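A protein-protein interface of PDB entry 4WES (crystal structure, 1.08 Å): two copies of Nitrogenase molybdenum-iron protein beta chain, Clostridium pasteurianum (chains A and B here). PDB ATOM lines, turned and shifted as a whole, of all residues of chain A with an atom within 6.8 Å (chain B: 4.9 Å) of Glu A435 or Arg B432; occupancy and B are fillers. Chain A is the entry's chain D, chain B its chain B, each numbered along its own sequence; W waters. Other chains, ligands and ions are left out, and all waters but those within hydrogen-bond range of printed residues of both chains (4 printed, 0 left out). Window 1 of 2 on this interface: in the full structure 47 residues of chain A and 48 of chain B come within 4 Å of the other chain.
Printed residues of chain B that touch a printed residue of chain A: Tyr B417, Gly B418, His B419, Asn B422, Lys B428, Arg B432 and Glu B435. Hydrophobic or aromatic side chains of chain B that line the printed part of chain A: Tyr B417. Along chain B the printed residues that touch a printed residue of chain A span positions 417 to 435. Of the 13 printed residues of chain A, 5 touch a printed residue of chain B. Among the printed residues, Asp or Glu carboxylates within 4 Å of a Lys or Arg side-chain nitrogen of the other chain: Glu A435 with Arg B432.
Asn A422 touches Arg B432, but with the chains exchanged Arg A432 does not touch Asn B422 (5.8 Å). Asn A422 touches Glu B435, and with the chains exchanged Glu A435 touches Asn B422. Glu A435 touches Arg B432, but with the chains exchanged Arg A432 does not touch Glu B435 (6.3 Å). Of the 10 pairs that touch across the chains among the printed residues, 2 have their exchanged pair printed and touching as well.
O of Gly B418 sits at hydrogen-bond distance from ND2 of Asn B422 (3.0 Å). O of His B419 lies close to OD1 of Asn B422. The guanidinium group of Arg B432 is in salt-bridge range of the side-chain carboxylate of Glu B435 (3.9 Å). OD1 of Asn A422 is in hydrogen-bond range of NH1 of Arg A432, at 2.8 Å. The backbone carbonyl oxygen (O) of Val A434 is in hydrogen-bond range of the side-chain hydroxyl (OG1) of Thr A438, 2.8 Å away. O of Glu A435 lies within hydrogen-bond range of OG1 of Thr A438, at 3.4 Å.
Of the printed residues of chain B, Asn A422 touches Arg B432 (3.3 Å) and Glu B435 (2.8 Å). Of the printed residues of chain B, Arg A432 touches Lys B428. Of the printed residues of chain B, Glu A435 touches Tyr B417, His B419, Asn B422 and Arg B432. Of the printed residues of chain B, Thr A438 touches Tyr B417 (3.99 Å). Of the printed residues of chain A, His B419 touches Glu A435 (3.7 Å). Of the printed residues of chain A, Lys B428 touches Arg A432. Of the printed residues of chain A, Arg B432 touches Asn A422 and Glu A435. The nearest printed residue of chain B that does not touch Glu A435 is Gly B418 (4.02 Å). The nearest printed residue of chain A that does not touch Arg B432 is Arg A432 (4.01 Å).
OD1 of Asn B422 sits close to OE2 of Glu A435 (3.4 Å). The guanidinium group of Arg B432 sits at hydrogen-bond distance from the side-chain amide oxygen of Asn A422 (3.3 Å). OE1 of Glu A435 is in salt-bridge range of NH2 of Arg B432. ND2 of Asn A422 lies within hydrogen-bond range of OE1 of Glu B435 (2.8 Å).
CD1 of Leu A302 touches CB of Tyr B417, at 3.8 Å. Leu A302 touches Gly B418. Lys B428 touches Arg A432 (CE to NH2, 3.9 Å). Glu A435 touches Tyr B417. Glu A435 touches His B419 (OE2 to CA, 3.7 Å). Thr A438 touches Tyr B417 (OG1 to CB, 3.99 Å).
Water W3 bridges the side-chain carboxylate of Glu A435 (2.7 Å) and the guanidinium group of Arg B432 (3.1 Å). Water W2 lies within hydrogen-bond range of OE1 of Glu A435 (2.7 Å), O of Gly B418 (2.9 Å) and ND2 of Asn B422 (2.9 Å). Water W4 lies within hydrogen-bond range of the side-chain amide oxygen (OD1) of Asn A439, the side-chain hydroxyl (OG1) of Thr A438 and the backbone NH (N) of Tyr B417. Water W1 bridges OE2 of Glu B436 and ND2 of Asn A439.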
ATOM      1  N   LEU A 302      31.334  -5.811  25.005  1.00  0.00           N
ATOM      2  CA  LEU A 302      31.862  -6.333  23.726  1.00  0.00           C
ATOM      3  C   LEU A 302      32.972  -5.439  23.200  1.00  0.00           C
ATOM      4  O   LEU A 302      34.012  -5.922  22.696  1.00  0.00           O
ATOM      5  CB  LEU A 302      30.732  -6.478  22.733  1.00  0.00           C
ATOM      6  CG  LEU A 302      31.123  -6.978  21.352  1.00  0.00           C
ATOM      7  CD1 LEU A 302      31.810  -8.342  21.397  1.00  0.00           C
ATOM      8  CD2 LEU A 302      29.903  -7.054  20.471  1.00  0.00           C
ATOM      9  N   ASN A 422      18.702  -7.576   9.890  1.00  0.00           N
ATOM     10  CA  ASN A 422      19.631  -7.164  10.961  1.00  0.00           C
ATOM     11  C   ASN A 422      19.701  -5.666  11.064  1.00  0.00           C
ATOM     12  O   ASN A 422      20.054  -4.984  10.102  1.00  0.00           O
ATOM     13  CB  ASN A 422      21.065  -7.630  10.660  1.00  0.00           C
ATOM     14  CG  ASN A 422      21.174  -9.147  10.553  1.00  0.00           C
ATOM     15  OD1 ASN A 422      20.668  -9.848  11.438  1.00  0.00           O
ATOM     16  ND2 ASN A 422      21.868  -9.656   9.508  1.00  0.00           N
ATOM     17  N   ALA A 430      24.634  -2.027  17.160  1.00  0.00           N
ATOM     18  CA  ALA A 430      26.057  -1.797  17.404  1.00  0.00           C
ATOM     19  C   ALA A 430      26.769  -3.100  17.739  1.00  0.00           C
ATOM     20  O   ALA A 430      27.893  -3.330  17.277  1.00  0.00           O
ATOM     21  CB  ALA A 430      26.229  -0.764  18.508  1.00  0.00           C
ATOM     22  N   ILE A 431      26.129  -3.930  18.559  1.00  0.00           N
ATOM     23  CA  ILE A 431      26.682  -5.239  18.905  1.00  0.00           C
ATOM     24  C   ILE A 431      26.892  -6.070  17.632  1.00  0.00           C
ATOM     25  O   ILE A 431      27.980  -6.666  17.405  1.00  0.00           O
ATOM     26  CB  ILE A 431      25.757  -5.954  19.909  1.00  0.00           C
ATOM     27  CG1 ILE A 431      25.894  -5.313  21.264  1.00  0.00           C
ATOM     28  CG2 ILE A 431      26.049  -7.463  19.939  1.00  0.00           C
ATOM     29  CD1 ILE A 431      24.831  -5.752  22.261  1.00  0.00           C
ATOM     30  N   ARG A 432      25.886  -6.079  16.763  1.00  0.00           N
ATOM     31  CA  ARG A 432      26.030  -6.788  15.487  1.00  0.00           C
ATOM     32  C   ARG A 432      27.182  -6.259  14.636  1.00  0.00           C
ATOM     33  O   ARG A 432      27.931  -7.051  14.036  1.00  0.00           O
ATOM     34  CB  ARG A 432      24.724  -6.752  14.702  1.00  0.00           C
ATOM     35  CG  ARG A 432      23.627  -7.552  15.372  1.00  0.00           C
ATOM     36  CD  ARG A 432      22.353  -7.927  14.624  1.00  0.00           C
ATOM     37  NE  ARG A 432      21.560  -8.773  15.538  1.00  0.00           N
ATOM     38  CZ  ARG A 432      20.429  -9.415  15.243  1.00  0.00           C
ATOM     39  NH1 ARG A 432      19.889  -9.339  14.029  1.00  0.00           N
ATOM     40  NH2 ARG A 432      19.840 -10.146  16.185  1.00  0.00           N
ATOM     41  N   LEU A 433      27.351  -4.948  14.590  1.00  0.00           N
ATOM     42  CA  LEU A 433      28.436  -4.356  13.838  1.00  0.00           C
ATOM     43  C   LEU A 433      29.782  -4.769  14.395  1.00  0.00           C
ATOM     44  O   LEU A 433      30.713  -5.055  13.625  1.00  0.00           O
ATOM     45  CB  LEU A 433      28.311  -2.831  13.835  1.00  0.00           C
ATOM     46  CG  LEU A 433      27.290  -2.241  12.879  1.00  0.00           C
ATOM     47  CD1 LEU A 433      27.112  -0.748  13.184  1.00  0.00           C
ATOM     48  CD2 LEU A 433      27.662  -2.440  11.422  1.00  0.00           C
ATOM     49  N   VAL A 434      29.953  -4.740  15.711  1.00  0.00           N
ATOM     50  CA  VAL A 434      31.245  -5.127  16.291  1.00  0.00           C
ATOM     51  C   VAL A 434      31.557  -6.580  15.996  1.00  0.00           C
ATOM     52  O   VAL A 434      32.715  -6.925  15.688  1.00  0.00           O
ATOM     53  CB  VAL A 434      31.341  -4.803  17.777  1.00  0.00           C
ATOM     54  CG1 VAL A 434      32.671  -5.239  18.357  1.00  0.00           C
ATOM     55  CG2 VAL A 434      31.124  -3.306  18.035  1.00  0.00           C
ATOM     56  N   GLU A 435      30.580  -7.438  16.141  1.00  0.00           N
ATOM     57  CA  GLU A 435      30.762  -8.837  15.773  1.00  0.00           C
ATOM     58  C   GLU A 435      31.186  -8.965  14.312  1.00  0.00           C
ATOM     59  O   GLU A 435      32.141  -9.692  14.000  1.00  0.00           O
ATOM     60  CB  GLU A 435      29.495  -9.648  16.034  1.00  0.00           C
ATOM     61  CG  GLU A 435      29.717 -11.116  15.722  1.00  0.00           C
ATOM     62  CD  GLU A 435      28.480 -11.966  15.788  1.00  0.00           C
ATOM     63  OE1 GLU A 435      27.354 -11.431  15.690  1.00  0.00           O
ATOM     64  OE2 GLU A 435      28.666 -13.209  15.840  1.00  0.00           O
ATOM     65  N   GLU A 436      30.489  -8.292  13.413  1.00  0.00           N
ATOM     66  CA  GLU A 436      30.802  -8.412  11.982  1.00  0.00           C
ATOM     67  C   GLU A 436      32.210  -7.896  11.684  1.00  0.00           C
ATOM     68  O   GLU A 436      32.973  -8.525  10.924  1.00  0.00           O
ATOM     69  CB  GLU A 436      29.781  -7.645  11.180  1.00  0.00           C
ATOM     70  CG  GLU A 436      29.835  -7.820   9.700  1.00  0.00           C
ATOM     71  CD  GLU A 436      28.612  -7.213   8.984  1.00  0.00           C
ATOM     72  OE1 GLU A 436      27.875  -6.311   9.561  1.00  0.00           O
ATOM     73  OE2 GLU A 436      28.406  -7.575   7.823  1.00  0.00           O
ATOM     74  N   ILE A 437      32.562  -6.742  12.237  1.00  0.00           N
ATOM     75  CA  ILE A 437      33.870  -6.150  12.006  1.00  0.00           C
ATOM     76  C   ILE A 437      34.968  -7.070  12.519  1.00  0.00           C
ATOM     77  O   ILE A 437      35.963  -7.336  11.820  1.00  0.00           O
ATOM     78  CB  ILE A 437      33.948  -4.747  12.685  1.00  0.00           C
ATOM     79  CG1 ILE A 437      33.077  -3.751  11.924  1.00  0.00           C
ATOM     80  CG2 ILE A 437      35.413  -4.302  12.784  1.00  0.00           C
ATOM     81  CD1 ILE A 437      32.844  -2.459  12.636  1.00  0.00           C
ATOM     82  N   THR A 438      34.837  -7.536  13.746  1.00  0.00           N
ATOM     83  CA  THR A 438      35.868  -8.388  14.291  1.00  0.00           C
ATOM     84  C   THR A 438      35.919  -9.748  13.621  1.00  0.00           C
ATOM     85  O   THR A 438      37.036 -10.300  13.425  1.00  0.00           O
ATOM     86  CB  THR A 438      35.789  -8.480  15.814  1.00  0.00           C
ATOM     87  OG1 THR A 438      34.572  -9.007  16.246  1.00  0.00           O
ATOM     88  CG2 THR A 438      35.969  -7.132  16.461  1.00  0.00           C
ATOM     89  N   ASN A 439      34.766 -10.265  13.208  1.00  0.00           N
ATOM     90  CA  ASN A 439      34.780 -11.514  12.448  1.00  0.00           C
ATOM     91  C   ASN A 439      35.601 -11.391  11.166  1.00  0.00           C
ATOM     92  O   ASN A 439      36.382 -12.296  10.836  1.00  0.00           O
ATOM     93  CB  ASN A 439      33.361 -11.946  12.052  1.00  0.00           C
ATOM     94  CG  ASN A 439      32.538 -12.612  13.154  1.00  0.00           C
ATOM     95  OD1 ASN A 439      33.014 -12.873  14.245  1.00  0.00           O
ATOM     96  ND2 ASN A 439      31.286 -12.932  12.818  1.00  0.00           N
ATOM     97  N   VAL A 440      35.391 -10.327  10.385  1.00  0.00           N
ATOM     98  CA  VAL A 440      36.105 -10.240   9.117  1.00  0.00           C
ATOM     99  C   VAL A 440      37.584 -10.006   9.329  1.00  0.00           C
ATOM    100  O   VAL A 440      38.427 -10.483   8.550  1.00  0.00           O
ATOM    101  CB  VAL A 440      35.476  -9.213   8.127  1.00  0.00           C
ATOM    102  CG1 VAL A 440      34.081  -9.611   7.723  1.00  0.00           C
ATOM    103  CG2 VAL A 440      35.543  -7.768   8.580  1.00  0.00           C
ATOM    104  N   TYR B 417      34.076 -12.913  18.808  1.00  0.00           N
ATOM    105  CA  TYR B 417      33.504 -11.980  19.794  1.00  0.00           C
ATOM    106  C   TYR B 417      32.079 -11.651  19.432  1.00  0.00           C
ATOM    107  O   TYR B 417      31.780 -11.161  18.357  1.00  0.00           O
ATOM    108  CB  TYR B 417      34.330 -10.700  19.854  1.00  0.00           C
ATOM    109  CG  TYR B 417      35.668 -11.003  20.476  1.00  0.00           C
ATOM    110  CD1 TYR B 417      35.880 -10.831  21.806  1.00  0.00           C
ATOM    111  CD2 TYR B 417      36.740 -11.502  19.722  1.00  0.00           C
ATOM    112  CE1 TYR B 417      37.054 -11.135  22.426  1.00  0.00           C
ATOM    113  CE2 TYR B 417      37.924 -11.846  20.334  1.00  0.00           C
ATOM    114  CZ  TYR B 417      38.109 -11.662  21.676  1.00  0.00           C
ATOM    115  OH  TYR B 417      39.277 -11.961  22.333  1.00  0.00           O
ATOM    116  N   GLY B 418      31.170 -11.876  20.387  1.00  0.00           N
ATOM    117  CA  GLY B 418      29.768 -11.535  20.233  1.00  0.00           C
ATOM    118  C   GLY B 418      28.848 -12.650  19.813  1.00  0.00           C
ATOM    119  O   GLY B 418      27.616 -12.460  19.767  1.00  0.00           O
ATOM    120  N   HIS B 419      29.391 -13.834  19.536  1.00  0.00           N
ATOM    121  CA  HIS B 419      28.585 -14.946  19.051  1.00  0.00           C
ATOM    122  C   HIS B 419      27.527 -15.321  20.080  1.00  0.00           C
ATOM    123  O   HIS B 419      26.430 -15.748  19.711  1.00  0.00           O
ATOM    124  CB  HIS B 419      29.458 -16.150  18.679  1.00  0.00           C
ATOM    125  CG  HIS B 419      30.203 -16.751  19.818  1.00  0.00           C
ATOM    126  ND1 HIS B 419      29.630 -17.686  20.642  1.00  0.00           N
ATOM    127  CD2 HIS B 419      31.463 -16.555  20.282  1.00  0.00           C
ATOM    128  CE1 HIS B 419      30.502 -18.036  21.571  1.00  0.00           C
ATOM    129  NE2 HIS B 419      31.620 -17.369  21.376  1.00  0.00           N
ATOM    130  N   ASN B 422      23.874 -14.146  19.913  1.00  0.00           N
ATOM    131  CA  ASN B 422      22.959 -14.566  18.854  1.00  0.00           C
ATOM    132  C   ASN B 422      22.376 -15.938  19.117  1.00  0.00           C
ATOM    133  O   ASN B 422      23.070 -16.923  19.356  1.00  0.00           O
ATOM    134  CB  ASN B 422      23.531 -14.502  17.422  1.00  0.00           C
ATOM    135  CG  ASN B 422      24.980 -14.069  17.361  1.00  0.00           C
ATOM    136  OD1 ASN B 422      25.813 -14.762  16.772  1.00  0.00           O
ATOM    137  ND2 ASN B 422      25.284 -12.900  17.923  1.00  0.00           N
ATOM    138  N   PRO B 423      21.034 -16.016  19.055  1.00  0.00           N
ATOM    139  CA  PRO B 423      20.425 -17.310  19.236  1.00  0.00           C
ATOM    140  C   PRO B 423      20.583 -18.159  17.984  1.00  0.00           C
ATOM    141  O   PRO B 423      20.686 -17.603  16.876  1.00  0.00           O
ATOM    142  CB  PRO B 423      18.937 -16.969  19.429  1.00  0.00           C
ATOM    143  CG  PRO B 423      18.741 -15.721  18.625  1.00  0.00           C
ATOM    144  CD  PRO B 423      20.042 -14.956  18.818  1.00  0.00           C
ATOM    145  N   LYS B 428      13.871 -16.874  14.674  1.00  0.00           N
ATOM    146  CA  LYS B 428      14.900 -15.848  14.681  1.00  0.00           C
ATOM    147  C   LYS B 428      16.308 -16.443  14.533  1.00  0.00           C
ATOM    148  O   LYS B 428      17.147 -15.970  13.759  1.00  0.00           O
ATOM    149  CB  LYS B 428      14.803 -15.067  15.994  1.00  0.00           C
ATOM    150  CG  LYS B 428      15.808 -13.959  16.217  1.00  0.00           C
ATOM    151  CD  LYS B 428      15.670 -13.141  17.511  1.00  0.00           C
ATOM    152  CE  LYS B 428      16.865 -12.182  17.599  1.00  0.00           C
ATOM    153  NZ  LYS B 428      17.058 -11.509  18.920  1.00  0.00           N
ATOM    154  N   GLY B 429      16.577 -17.485  15.304  1.00  0.00           N
ATOM    155  CA  GLY B 429      17.864 -18.151  15.244  1.00  0.00           C
ATOM    156  C   GLY B 429      18.075 -18.860  13.923  1.00  0.00           C
ATOM    157  O   GLY B 429      19.189 -18.884  13.376  1.00  0.00           O
ATOM    158  N   ALA B 430      17.011 -19.426  13.358  1.00  0.00           N
ATOM    159  CA  ALA B 430      17.099 -20.081  12.063  1.00  0.00           C
ATOM    160  C   ALA B 430      17.462 -19.089  10.964  1.00  0.00           C
ATOM    161  O   ALA B 430      18.260 -19.411  10.077  1.00  0.00           O
ATOM    162  CB  ALA B 430      15.780 -20.773  11.738  1.00  0.00           C
ATOM    163  N   ILE B 431      16.881 -17.892  11.018  1.00  0.00           N
ATOM    164  CA  ILE B 431      17.213 -16.843  10.064  1.00  0.00           C
ATOM    165  C   ILE B 431      18.703 -16.526  10.153  1.00  0.00           C
ATOM    166  O   ILE B 431      19.400 -16.405   9.137  1.00  0.00           O
ATOM    167  CB  ILE B 431      16.327 -15.598  10.324  1.00  0.00           C
ATOM    168  CG1 ILE B 431      14.902 -15.893   9.854  1.00  0.00           C
ATOM    169  CG2 ILE B 431      16.897 -14.342   9.663  1.00  0.00           C
ATOM    170  CD1 ILE B 431      13.868 -14.859  10.371  1.00  0.00           C
ATOM    171  N   ARG B 432      19.214 -16.362  11.370  1.00  0.00           N
ATOM    172  CA  ARG B 432      20.632 -16.073  11.555  1.00  0.00           C
ATOM    173  C   ARG B 432      21.503 -17.176  10.997  1.00  0.00           C
ATOM    174  O   ARG B 432      22.538 -16.908  10.350  1.00  0.00           O
ATOM    175  CB  ARG B 432      20.938 -15.857  13.029  1.00  0.00           C
ATOM    176  CG  ARG B 432      20.337 -14.581  13.621  1.00  0.00           C
ATOM    177  CD  ARG B 432      21.164 -13.328  13.320  1.00  0.00           C
ATOM    178  NE  ARG B 432      22.573 -13.445  13.705  1.00  0.00           N
ATOM    179  CZ  ARG B 432      23.514 -12.531  13.457  1.00  0.00           C
ATOM    180  NH1 ARG B 432      23.228 -11.396  12.823  1.00  0.00           N
ATOM    181  NH2 ARG B 432      24.760 -12.757  13.847  1.00  0.00           N
ATOM    182  N   LEU B 433      21.112 -18.434  11.196  1.00  0.00           N
ATOM    183  CA  LEU B 433      21.861 -19.571  10.650  1.00  0.00           C
ATOM    184  C   LEU B 433      21.886 -19.562   9.129  1.00  0.00           C
ATOM    185  O   LEU B 433      22.939 -19.819   8.519  1.00  0.00           O
ATOM    186  CB  LEU B 433      21.293 -20.897  11.158  1.00  0.00           C
ATOM    187  CG  LEU B 433      21.647 -21.272  12.586  1.00  0.00           C
ATOM    188  CD1 LEU B 433      20.796 -22.449  13.028  1.00  0.00           C
ATOM    189  CD2 LEU B 433      23.141 -21.553  12.752  1.00  0.00           C
ATOM    190  N   VAL B 434      20.744 -19.312   8.480  1.00  0.00           N
ATOM    191  CA  VAL B 434      20.748 -19.309   7.037  1.00  0.00           C
ATOM    192  C   VAL B 434      21.611 -18.191   6.480  1.00  0.00           C
ATOM    193  O   VAL B 434      22.345 -18.381   5.513  1.00  0.00           O
ATOM    194  CB  VAL B 434      19.323 -19.210   6.447  1.00  0.00           C
ATOM    195  CG1 VAL B 434      19.327 -19.159   4.933  1.00  0.00           C
ATOM    196  CG2 VAL B 434      18.491 -20.399   6.952  1.00  0.00           C
ATOM    197  N   GLU B 435      21.553 -17.018   7.097  1.00  0.00           N
ATOM    198  CA  GLU B 435      22.434 -15.926   6.703  1.00  0.00           C
ATOM    199  C   GLU B 435      23.902 -16.315   6.850  1.00  0.00           C
ATOM    200  O   GLU B 435      24.699 -16.092   5.941  1.00  0.00           O
ATOM    201  CB  GLU B 435      22.120 -14.673   7.508  1.00  0.00           C
ATOM    202  CG  GLU B 435      22.989 -13.514   7.092  1.00  0.00           C
ATOM    203  CD  GLU B 435      22.897 -12.291   7.934  1.00  0.00           C
ATOM    204  OE1 GLU B 435      22.459 -12.384   9.127  1.00  0.00           O
ATOM    205  OE2 GLU B 435      23.310 -11.232   7.427  1.00  0.00           O
ATOM    206  N   GLU B 436      24.238 -16.889   7.997  1.00  0.00           N
ATOM    207  CA  GLU B 436      25.642 -17.264   8.216  1.00  0.00           C
ATOM    208  C   GLU B 436      26.131 -18.318   7.238  1.00  0.00           C
ATOM    209  O   GLU B 436      27.235 -18.224   6.698  1.00  0.00           O
ATOM    210  CB  GLU B 436      25.805 -17.781   9.635  1.00  0.00           C
ATOM    211  CG  GLU B 436      27.214 -17.968  10.104  1.00  0.00           C
ATOM    212  CD  GLU B 436      27.275 -18.251  11.621  1.00  0.00           C
ATOM    213  OE1 GLU B 436      26.246 -18.692  12.267  1.00  0.00           O
ATOM    214  OE2 GLU B 436      28.372 -18.096  12.169  1.00  0.00           O
HETATM  215  O   HOH W   1      29.468 -15.553  11.873  1.00  0.00           O
HETATM  216  O   HOH W   2      26.638 -10.328  18.100  1.00  0.00           O
HETATM  217  O   HOH W   3      27.423 -14.316  13.660  1.00  0.00           O
HETATM  218  O   HOH W   4      34.607 -11.796  16.259  1.00  0.00           O
